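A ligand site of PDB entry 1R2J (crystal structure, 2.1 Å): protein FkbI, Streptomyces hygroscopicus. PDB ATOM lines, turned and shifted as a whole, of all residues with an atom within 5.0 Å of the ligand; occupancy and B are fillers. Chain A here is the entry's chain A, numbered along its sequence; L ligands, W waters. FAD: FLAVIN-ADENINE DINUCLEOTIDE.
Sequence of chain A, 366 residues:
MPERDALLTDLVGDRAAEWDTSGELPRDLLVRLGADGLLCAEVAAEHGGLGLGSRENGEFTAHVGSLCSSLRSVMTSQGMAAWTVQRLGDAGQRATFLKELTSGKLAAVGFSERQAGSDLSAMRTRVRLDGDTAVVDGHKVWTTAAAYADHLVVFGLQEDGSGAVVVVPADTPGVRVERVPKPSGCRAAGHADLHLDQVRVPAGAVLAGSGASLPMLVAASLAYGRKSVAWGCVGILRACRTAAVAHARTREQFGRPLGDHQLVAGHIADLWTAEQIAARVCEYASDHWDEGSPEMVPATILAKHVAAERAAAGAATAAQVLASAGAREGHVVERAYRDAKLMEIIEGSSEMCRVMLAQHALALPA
N5 of the ligand sits close to O of Trp 142 (3.0 Å).
Residues that only touch the ligand: Gly 110 (3.98 Å), Thr 143 (3.8 Å), His 191 (3.4 Å), Leu 342 (3.5 Å), Ile 346 (3.5 Å) and Met 352 (3.9 Å).
Hydrophobic or aromatic side chains that line the ligand: Phe 111, Trp 142, His 191, Leu 342, Ile 345, Ile 346 and Met 352.
Water W6 bridges O of Gly 117 (2.8 Å) and O4' of the ligand (3.0 Å).
Water W3 lies within hydrogen-bond range of the backbone NH (N) of Val 109, the side-chain hydroxyl (OG) of Ser 77, the backbone carbonyl oxygen (O) of Thr 144 and an oxygen (O4) of the ligand.
Water W5 bridges the backbone NH (N) of Glu 347 (3.1 Å) and an oxygen (O2') of the ligand (3.1 Å).
Water W1 lies within hydrogen-bond range of OG1 of Thr 143 (2.7 Å), O of Val 141 (2.8 Å) and O2 of the ligand (3.3 Å).
Water W2 bridges the side-chain carboxylate (OE1) of Glu 347 (3.0 Å) and an oxygen (O4) of the ligand (3.3 Å).
The side-chain hydroxyl (OG) of Ser 349 sits close to the backbone NH (N) of Glu 351.
N of Met 352 sits at hydrogen-bond distance from OG of Ser 349 (3.1 Å).
O of Thr 144 lies close to OG of Ser 77, at 3.5 Å.
The backbone carbonyl oxygen (O) of Ser 112 lies within hydrogen-bond range of the backbone NH (N) of Val 141 (3.0 Å).
OG of Ser 112 is in hydrogen-bond range of O of Ala 116.
NE2 of His 191 sits at hydrogen-bond distance from O of Cys 186 (2.8 Å).
The side-chain hydroxyl of Ser 349 is in hydrogen-bond range of an oxygen (O2B) of the ligand, at 2.5 Å.
The backbone NH (N) of Thr 144 sits at hydrogen-bond distance from an oxygen (O4) of the ligand, 2.9 Å away.
N5 of the ligand lies within hydrogen-bond range of OG1 of Thr 144 (2.6 Å).
An oxygen (O2B) of the ligand lies within hydrogen-bond range of the side-chain carboxylate of Glu 351, at 2.7 Å.
An oxygen (O1A) of the ligand sits at hydrogen-bond distance from the backbone NH of Ser 118.
OG of Ser 118 is in hydrogen-bond range of O1A of the ligand, at 2.8 Å.
The backbone NH (N) of Ser 112 sits at hydrogen-bond distance from an oxygen (O2) of the ligand (2.9 Å).
A nitrogen (N3) of the ligand lies within hydrogen-bond range of the backbone carbonyl oxygen (O) of Val 109.
The backbone carbonyl oxygen of Gly 117 sits close to an oxygen (O4') of the ligand, at 3.2 Å.
The backbone NH (N) of Phe 111 lies within hydrogen-bond range of an oxygen (O2) of the ligand (3.0 Å).
The backbone carbonyl oxygen (O) of Ile 345 lies close to an oxygen (O3') of the ligand (3.5 Å).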
ATOM      1  N   SER A  77       1.865   7.727   7.255  1.00  0.00           N
ATOM      2  CA  SER A  77       1.684   6.306   7.030  1.00  0.00           C
ATOM      3  C   SER A  77       2.503   5.866   5.810  1.00  0.00           C
ATOM      4  O   SER A  77       3.193   4.844   5.842  1.00  0.00           O
ATOM      5  CB  SER A  77       0.208   5.988   6.799  1.00  0.00           C
ATOM      6  OG  SER A  77      -0.546   6.252   7.968  1.00  0.00           O
ATOM      7  N   VAL A 109       0.403   1.136   7.721  1.00  0.00           N
ATOM      8  CA  VAL A 109       1.197   0.312   8.616  1.00  0.00           C
ATOM      9  C   VAL A 109       0.357  -0.054   9.839  1.00  0.00           C
ATOM     10  O   VAL A 109      -0.024   0.825  10.611  1.00  0.00           O
ATOM     11  CB  VAL A 109       2.457   1.071   9.077  1.00  0.00           C
ATOM     12  CG1 VAL A 109       3.397   0.120   9.801  1.00  0.00           C
ATOM     13  CG2 VAL A 109       3.133   1.714   7.877  1.00  0.00           C
ATOM     14  N   GLY A 110       0.087  -1.333  10.029  1.00  0.00           N
ATOM     15  CA  GLY A 110      -0.710  -1.763  11.166  1.00  0.00           C
ATOM     16  C   GLY A 110       0.034  -2.703  12.094  1.00  0.00           C
ATOM     17  O   GLY A 110       0.453  -3.793  11.688  1.00  0.00           O
ATOM     18  N   PHE A 111       0.205  -2.280  13.341  1.00  0.00           N
ATOM     19  CA  PHE A 111       0.876  -3.102  14.342  1.00  0.00           C
ATOM     20  C   PHE A 111       0.011  -3.175  15.592  1.00  0.00           C
ATOM     21  O   PHE A 111       0.031  -4.160  16.324  1.00  0.00           O
ATOM     22  CB  PHE A 111       2.263  -2.529  14.666  1.00  0.00           C
ATOM     23  CG  PHE A 111       2.307  -1.028  14.806  1.00  0.00           C
ATOM     24  CD1 PHE A 111       1.975  -0.416  16.009  1.00  0.00           C
ATOM     25  CD2 PHE A 111       2.657  -0.222  13.720  1.00  0.00           C
ATOM     26  CE1 PHE A 111       1.997   0.984  16.140  1.00  0.00           C
ATOM     27  CE2 PHE A 111       2.681   1.165  13.834  1.00  0.00           C
ATOM     28  CZ  PHE A 111       2.359   1.780  15.047  1.00  0.00           C
ATOM     29  N   SER A 112      -0.756  -2.127  15.827  1.00  0.00           N
ATOM     30  CA  SER A 112      -1.623  -2.074  16.987  1.00  0.00           C
ATOM     31  C   SER A 112      -2.790  -3.067  16.930  1.00  0.00           C
ATOM     32  O   SER A 112      -3.312  -3.360  15.855  1.00  0.00           O
ATOM     33  CB  SER A 112      -2.173  -0.666  17.163  1.00  0.00           C
ATOM     34  OG  SER A 112      -3.143  -0.663  18.186  1.00  0.00           O
ATOM     35  N   ALA A 116      -3.324  -4.798  22.346  1.00  0.00           N
ATOM     36  CA  ALA A 116      -1.947  -4.329  22.313  1.00  0.00           C
ATOM     37  C   ALA A 116      -1.866  -2.907  21.765  1.00  0.00           C
ATOM     38  O   ALA A 116      -1.841  -2.702  20.552  1.00  0.00           O
ATOM     39  CB  ALA A 116      -1.076  -5.272  21.453  1.00  0.00           C
ATOM     40  N   GLY A 117      -1.850  -1.923  22.675  1.00  0.00           N
ATOM     41  CA  GLY A 117      -1.774  -0.529  22.277  1.00  0.00           C
ATOM     42  C   GLY A 117      -0.402   0.016  22.626  1.00  0.00           C
ATOM     43  O   GLY A 117       0.507   0.008  21.807  1.00  0.00           O
ATOM     44  N   SER A 118      -0.261   0.491  23.850  1.00  0.00           N
ATOM     45  CA  SER A 118       1.025   1.011  24.294  1.00  0.00           C
ATOM     46  C   SER A 118       1.980  -0.180  24.416  1.00  0.00           C
ATOM     47  O   SER A 118       3.185  -0.036  24.243  1.00  0.00           O
ATOM     48  CB  SER A 118       0.878   1.721  25.637  1.00  0.00           C
ATOM     49  OG  SER A 118       0.041   2.872  25.519  1.00  0.00           O
ATOM     50  N   VAL A 141      -5.994  -2.714  14.629  1.00  0.00           N
ATOM     51  CA  VAL A 141      -6.999  -1.699  14.872  1.00  0.00           C
ATOM     52  C   VAL A 141      -6.487  -0.304  14.533  1.00  0.00           C
ATOM     53  O   VAL A 141      -5.281  -0.061  14.522  1.00  0.00           O
ATOM     54  CB  VAL A 141      -7.444  -1.683  16.345  1.00  0.00           C
ATOM     55  CG1 VAL A 141      -8.134  -2.995  16.688  1.00  0.00           C
ATOM     56  CG2 VAL A 141      -6.239  -1.445  17.259  1.00  0.00           C
ATOM     57  N   TRP A 142      -7.417   0.590  14.232  1.00  0.00           N
ATOM     58  CA  TRP A 142      -7.098   1.987  13.926  1.00  0.00           C
ATOM     59  C   TRP A 142      -5.995   2.251  12.911  1.00  0.00           C
ATOM     60  O   TRP A 142      -5.333   3.279  12.989  1.00  0.00           O
ATOM     61  CB  TRP A 142      -6.730   2.718  15.215  1.00  0.00           C
ATOM     62  CG  TRP A 142      -7.897   3.182  15.963  1.00  0.00           C
ATOM     63  CD1 TRP A 142      -8.577   2.507  16.934  1.00  0.00           C
ATOM     64  CD2 TRP A 142      -8.550   4.443  15.808  1.00  0.00           C
ATOM     65  NE1 TRP A 142      -9.617   3.274  17.394  1.00  0.00           N
ATOM     66  CE2 TRP A 142      -9.627   4.475  16.727  1.00  0.00           C
ATOM     67  CE3 TRP A 142      -8.330   5.557  14.986  1.00  0.00           C
ATOM     68  CZ2 TRP A 142     -10.474   5.572  16.836  1.00  0.00           C
ATOM     69  CZ3 TRP A 142      -9.175   6.645  15.097  1.00  0.00           C
ATOM     70  CH2 TRP A 142     -10.237   6.650  16.023  1.00  0.00           C
ATOM     71  N   THR A 143      -5.793   1.351  11.962  1.00  0.00           N
ATOM     72  CA  THR A 143      -4.748   1.545  10.960  1.00  0.00           C
ATOM     73  C   THR A 143      -4.996   2.767  10.083  1.00  0.00           C
ATOM     74  O   THR A 143      -5.968   2.807   9.324  1.00  0.00           O
ATOM     75  CB  THR A 143      -4.616   0.309  10.061  1.00  0.00           C
ATOM     76  OG1 THR A 143      -4.602  -0.865  10.886  1.00  0.00           O
ATOM     77  CG2 THR A 143      -3.323   0.367   9.265  1.00  0.00           C
ATOM     78  N   THR A 144      -4.126   3.769  10.196  1.00  0.00           N
ATOM     79  CA  THR A 144      -4.262   4.993   9.416  1.00  0.00           C
ATOM     80  C   THR A 144      -4.096   4.782   7.912  1.00  0.00           C
ATOM     81  O   THR A 144      -3.206   4.054   7.467  1.00  0.00           O
ATOM     82  CB  THR A 144      -3.219   6.048   9.843  1.00  0.00           C
ATOM     83  OG1 THR A 144      -3.454   6.412  11.208  1.00  0.00           O
ATOM     84  CG2 THR A 144      -3.337   7.285   8.969  1.00  0.00           C
ATOM     85  N   GLY A 185     -10.818  12.574  15.635  1.00  0.00           N
ATOM     86  CA  GLY A 185      -9.959  13.541  14.966  1.00  0.00           C
ATOM     87  C   GLY A 185      -9.303  12.934  13.746  1.00  0.00           C
ATOM     88  O   GLY A 185      -9.420  11.717  13.539  1.00  0.00           O
ATOM     89  N   CYS A 186      -8.608  13.744  12.941  1.00  0.00           N
ATOM     90  CA  CYS A 186      -7.983  13.245  11.715  1.00  0.00           C
ATOM     91  C   CYS A 186      -9.029  12.381  10.989  1.00  0.00           C
ATOM     92  O   CYS A 186      -8.726  11.366  10.367  1.00  0.00           O
ATOM     93  CB  CYS A 186      -6.746  12.400  12.071  1.00  0.00           C
ATOM     94  SG  CYS A 186      -5.257  13.347  12.572  1.00  0.00           S
ATOM     95  N   HIS A 191      -8.976   5.779   8.726  1.00  0.00           N
ATOM     96  CA  HIS A 191      -8.621   4.795   9.739  1.00  0.00           C
ATOM     97  C   HIS A 191      -9.498   3.562   9.533  1.00  0.00           C
ATOM     98  O   HIS A 191     -10.669   3.681   9.188  1.00  0.00           O
ATOM     99  CB  HIS A 191      -8.901   5.348  11.142  1.00  0.00           C
ATOM    100  CG  HIS A 191      -8.367   6.729  11.361  1.00  0.00           C
ATOM    101  ND1 HIS A 191      -7.022   6.988  11.486  1.00  0.00           N
ATOM    102  CD2 HIS A 191      -8.997   7.917  11.418  1.00  0.00           C
ATOM    103  CE1 HIS A 191      -6.840   8.293  11.615  1.00  0.00           C
ATOM    104  NE2 HIS A 191      -8.029   8.885  11.574  1.00  0.00           N
ATOM    105  N   LEU A 342      -5.348  13.898  19.705  1.00  0.00           N
ATOM    106  CA  LEU A 342      -5.013  12.550  19.240  1.00  0.00           C
ATOM    107  C   LEU A 342      -3.507  12.336  19.128  1.00  0.00           C
ATOM    108  O   LEU A 342      -3.009  11.248  19.433  1.00  0.00           O
ATOM    109  CB  LEU A 342      -5.703  12.288  17.894  1.00  0.00           C
ATOM    110  CG  LEU A 342      -6.894  11.316  17.903  1.00  0.00           C
ATOM    111  CD1 LEU A 342      -7.709  11.468  19.176  1.00  0.00           C
ATOM    112  CD2 LEU A 342      -7.761  11.559  16.672  1.00  0.00           C
ATOM    113  N   ILE A 345      -1.754  11.030  22.090  1.00  0.00           N
ATOM    114  CA  ILE A 345      -2.052   9.628  22.357  1.00  0.00           C
ATOM    115  C   ILE A 345      -1.301   8.624  21.465  1.00  0.00           C
ATOM    116  O   ILE A 345      -0.864   7.589  21.960  1.00  0.00           O
ATOM    117  CB  ILE A 345      -3.584   9.393  22.219  1.00  0.00           C
ATOM    118  CG1 ILE A 345      -4.344  10.231  23.260  1.00  0.00           C
ATOM    119  CG2 ILE A 345      -3.916   7.903  22.360  1.00  0.00           C
ATOM    120  CD1 ILE A 345      -5.821  10.463  22.928  1.00  0.00           C
ATOM    121  N   ILE A 346      -1.152   8.928  20.174  1.00  0.00           N
ATOM    122  CA  ILE A 346      -0.479   8.014  19.238  1.00  0.00           C
ATOM    123  C   ILE A 346       1.043   8.147  19.122  1.00  0.00           C
ATOM    124  O   ILE A 346       1.638   9.092  19.615  1.00  0.00           O
ATOM    125  CB  ILE A 346      -1.082   8.156  17.806  1.00  0.00           C
ATOM    126  CG1 ILE A 346      -0.482   9.362  17.072  1.00  0.00           C
ATOM    127  CG2 ILE A 346      -2.572   8.341  17.914  1.00  0.00           C
ATOM    128  CD1 ILE A 346      -0.926   9.470  15.593  1.00  0.00           C
ATOM    129  N   GLU A 347       1.656   7.167  18.444  1.00  0.00           N
ATOM    130  CA  GLU A 347       3.101   7.115  18.222  1.00  0.00           C
ATOM    131  C   GLU A 347       3.869   7.229  19.543  1.00  0.00           C
ATOM    132  O   GLU A 347       4.889   7.919  19.630  1.00  0.00           O
ATOM    133  CB  GLU A 347       3.534   8.237  17.264  1.00  0.00           C
ATOM    134  CG  GLU A 347       2.939   8.116  15.860  1.00  0.00           C
ATOM    135  CD  GLU A 347       3.718   7.179  14.964  1.00  0.00           C
ATOM    136  OE1 GLU A 347       3.229   6.873  13.852  1.00  0.00           O
ATOM    137  OE2 GLU A 347       4.816   6.744  15.355  1.00  0.00           O
ATOM    138  N   SER A 349       2.366   7.376  23.442  1.00  0.00           N
ATOM    139  CA  SER A 349       1.611   8.355  24.227  1.00  0.00           C
ATOM    140  C   SER A 349       2.516   9.213  25.092  1.00  0.00           C
ATOM    141  O   SER A 349       3.663   8.847  25.378  1.00  0.00           O
ATOM    142  CB  SER A 349       0.624   7.640  25.142  1.00  0.00           C
ATOM    143  OG  SER A 349       1.309   7.062  26.244  1.00  0.00           O
ATOM    144  N   GLU A 351       2.499   9.531  28.117  1.00  0.00           N
ATOM    145  CA  GLU A 351       2.942   8.727  29.248  1.00  0.00           C
ATOM    146  C   GLU A 351       4.099   7.825  28.874  1.00  0.00           C
ATOM    147  O   GLU A 351       5.070   7.738  29.613  1.00  0.00           O
ATOM    148  CB  GLU A 351       1.797   7.885  29.825  1.00  0.00           C
ATOM    149  CG  GLU A 351       0.727   8.694  30.541  1.00  0.00           C
ATOM    150  CD  GLU A 351       0.011   9.650  29.611  1.00  0.00           C
ATOM    151  OE1 GLU A 351      -0.406   9.177  28.528  1.00  0.00           O
ATOM    152  OE2 GLU A 351      -0.123  10.851  29.953  1.00  0.00           O
ATOM    153  N   MET A 352       4.005   7.149  27.738  1.00  0.00           N
ATOM    154  CA  MET A 352       5.077   6.269  27.304  1.00  0.00           C
ATOM    155  C   MET A 352       6.330   7.080  26.954  1.00  0.00           C
ATOM    156  O   MET A 352       7.451   6.633  27.185  1.00  0.00           O
ATOM    157  CB  MET A 352       4.637   5.429  26.097  1.00  0.00           C
ATOM    158  CG  MET A 352       3.570   4.390  26.435  1.00  0.00           C
ATOM    159  SD  MET A 352       3.997   3.446  27.924  1.00  0.00           S
ATOM    160  CE  MET A 352       5.299   2.426  27.286  1.00  0.00           C
ATOM    161  N   VAL A 355       8.037   7.752  30.162  1.00  0.00           N
ATOM    162  CA  VAL A 355       8.770   6.606  30.705  1.00  0.00           C
ATOM    163  C   VAL A 355      10.047   6.368  29.902  1.00  0.00           C
ATOM    164  O   VAL A 355      11.093   6.047  30.470  1.00  0.00           O
ATOM    165  CB  VAL A 355       7.928   5.287  30.735  1.00  0.00           C
ATOM    166  CG1 VAL A 355       6.565   5.548  31.344  1.00  0.00           C
ATOM    167  CG2 VAL A 355       7.817   4.708  29.351  1.00  0.00           C
HETATM  168  PA  FAD L   1      -3.719   1.975  26.125  1.00  0.00           P
HETATM  169  O1A FAD L   1      -2.531   1.780  25.309  1.00  0.00           O
HETATM  170  O2A FAD L   1      -4.973   1.172  26.330  1.00  0.00           O
HETATM  171  O5B FAD L   1      -4.092   3.417  26.486  1.00  0.00           O
HETATM  172  C5B FAD L   1      -3.556   3.576  27.736  1.00  0.00           C
HETATM  173  C4B FAD L   1      -3.673   4.899  28.411  1.00  0.00           C
HETATM  174  O4B FAD L   1      -2.883   4.411  29.548  1.00  0.00           O
HETATM  175  C3B FAD L   1      -2.797   5.877  27.689  1.00  0.00           C
HETATM  176  O3B FAD L   1      -3.141   7.166  28.085  1.00  0.00           O
HETATM  177  C2B FAD L   1      -1.448   5.519  28.074  1.00  0.00           C
HETATM  178  O2B FAD L   1      -0.382   6.505  28.005  1.00  0.00           O
HETATM  179  C1B FAD L   1      -1.591   4.958  29.515  1.00  0.00           C
HETATM  180  N9A FAD L   1      -0.644   3.921  29.767  1.00  0.00           N
HETATM  181  C8A FAD L   1      -0.528   2.604  29.254  1.00  0.00           C
HETATM  182  N7A FAD L   1       0.485   1.913  29.688  1.00  0.00           N
HETATM  183  C5A FAD L   1       1.125   2.776  30.561  1.00  0.00           C
HETATM  184  C6A FAD L   1       2.265   2.653  31.366  1.00  0.00           C
HETATM  185  N6A FAD L   1       2.995   1.527  31.413  1.00  0.00           N
HETATM  186  N1A FAD L   1       2.640   3.733  32.128  1.00  0.00           N
HETATM  187  C2A FAD L   1       1.916   4.886  32.106  1.00  0.00           C
HETATM  188  N3A FAD L   1       0.768   5.102  31.351  1.00  0.00           N
HETATM  189  C4A FAD L   1       0.472   3.926  30.605  1.00  0.00           C
HETATM  190  N1  FAD L   1      -1.898   2.127  15.386  1.00  0.00           N
HETATM  191  C2  FAD L   1      -1.198   1.497  14.347  1.00  0.00           C
HETATM  192  O2  FAD L   1      -0.636   0.397  14.504  1.00  0.00           O
HETATM  193  N3  FAD L   1      -1.134   2.100  13.109  1.00  0.00           N
HETATM  194  C4  FAD L   1      -1.742   3.338  12.776  1.00  0.00           C
HETATM  195  O4  FAD L   1      -1.634   3.808  11.600  1.00  0.00           O
HETATM  196  C4X FAD L   1      -2.447   3.933  13.802  1.00  0.00           C
HETATM  197  N5  FAD L   1      -3.100   5.196  13.473  1.00  0.00           N
HETATM  198  C5X FAD L   1      -3.852   5.831  14.488  1.00  0.00           C
HETATM  199  C6  FAD L   1      -4.547   7.044  14.249  1.00  0.00           C
HETATM  200  C7  FAD L   1      -5.355   7.702  15.226  1.00  0.00           C
HETATM  201  C7M FAD L   1      -6.068   9.013  14.883  1.00  0.00           C
HETATM  202  C8  FAD L   1      -5.488   7.095  16.503  1.00  0.00           C
HETATM  203  C8M FAD L   1      -6.341   7.662  17.621  1.00  0.00           C
HETATM  204  C9  FAD L   1      -4.823   5.930  16.791  1.00  0.00           C
HETATM  205  C9A FAD L   1      -3.976   5.279  15.814  1.00  0.00           C
HETATM  206  N10 FAD L   1      -3.249   4.005  16.078  1.00  0.00           N
HETATM  207  C10 FAD L   1      -2.508   3.322  15.094  1.00  0.00           C
HETATM  208  C1' FAD L   1      -3.416   3.679  17.425  1.00  0.00           C
HETATM  209  C2' FAD L   1      -2.246   4.321  18.359  1.00  0.00           C
HETATM  210  O2' FAD L   1      -1.212   3.313  18.168  1.00  0.00           O
HETATM  211  C3' FAD L   1      -2.742   4.179  19.681  1.00  0.00           C
HETATM  212  O3' FAD L   1      -3.051   5.493  20.206  1.00  0.00           O
HETATM  213  C4' FAD L   1      -2.110   3.557  20.955  1.00  0.00           C
HETATM  214  O4' FAD L   1      -1.478   2.305  20.892  1.00  0.00           O
HETATM  215  C5' FAD L   1      -3.370   3.487  21.673  1.00  0.00           C
HETATM  216  O5' FAD L   1      -3.519   2.367  22.500  1.00  0.00           O
HETATM  217  P   FAD L   1      -4.985   2.200  23.149  1.00  0.00           P
HETATM  218  O1P FAD L   1      -4.278   1.038  22.915  1.00  0.00           O
HETATM  219  O2P FAD L   1      -5.980   1.259  23.898  1.00  0.00           O
HETATM  220  O3P FAD L   1      -4.453   2.112  24.689  1.00  0.00           O
HETATM  221  O   HOH W   1      -3.142  -1.137  13.093  1.00  0.00           O
HETATM  222  O   HOH W   2       0.850   5.960  12.227  1.00  0.00           O
HETATM  223  O   HOH W   3      -0.672   3.491   8.719  1.00  0.00           O
HETATM  224  O   HOH W   4      -7.772   3.546  23.916  1.00  0.00           O
HETATM  225  O   HOH W   5       0.794   4.953  16.416  1.00  0.00           O
HETATM  226  O   HOH W   6       0.656   1.039  19.186  1.00  0.00           O
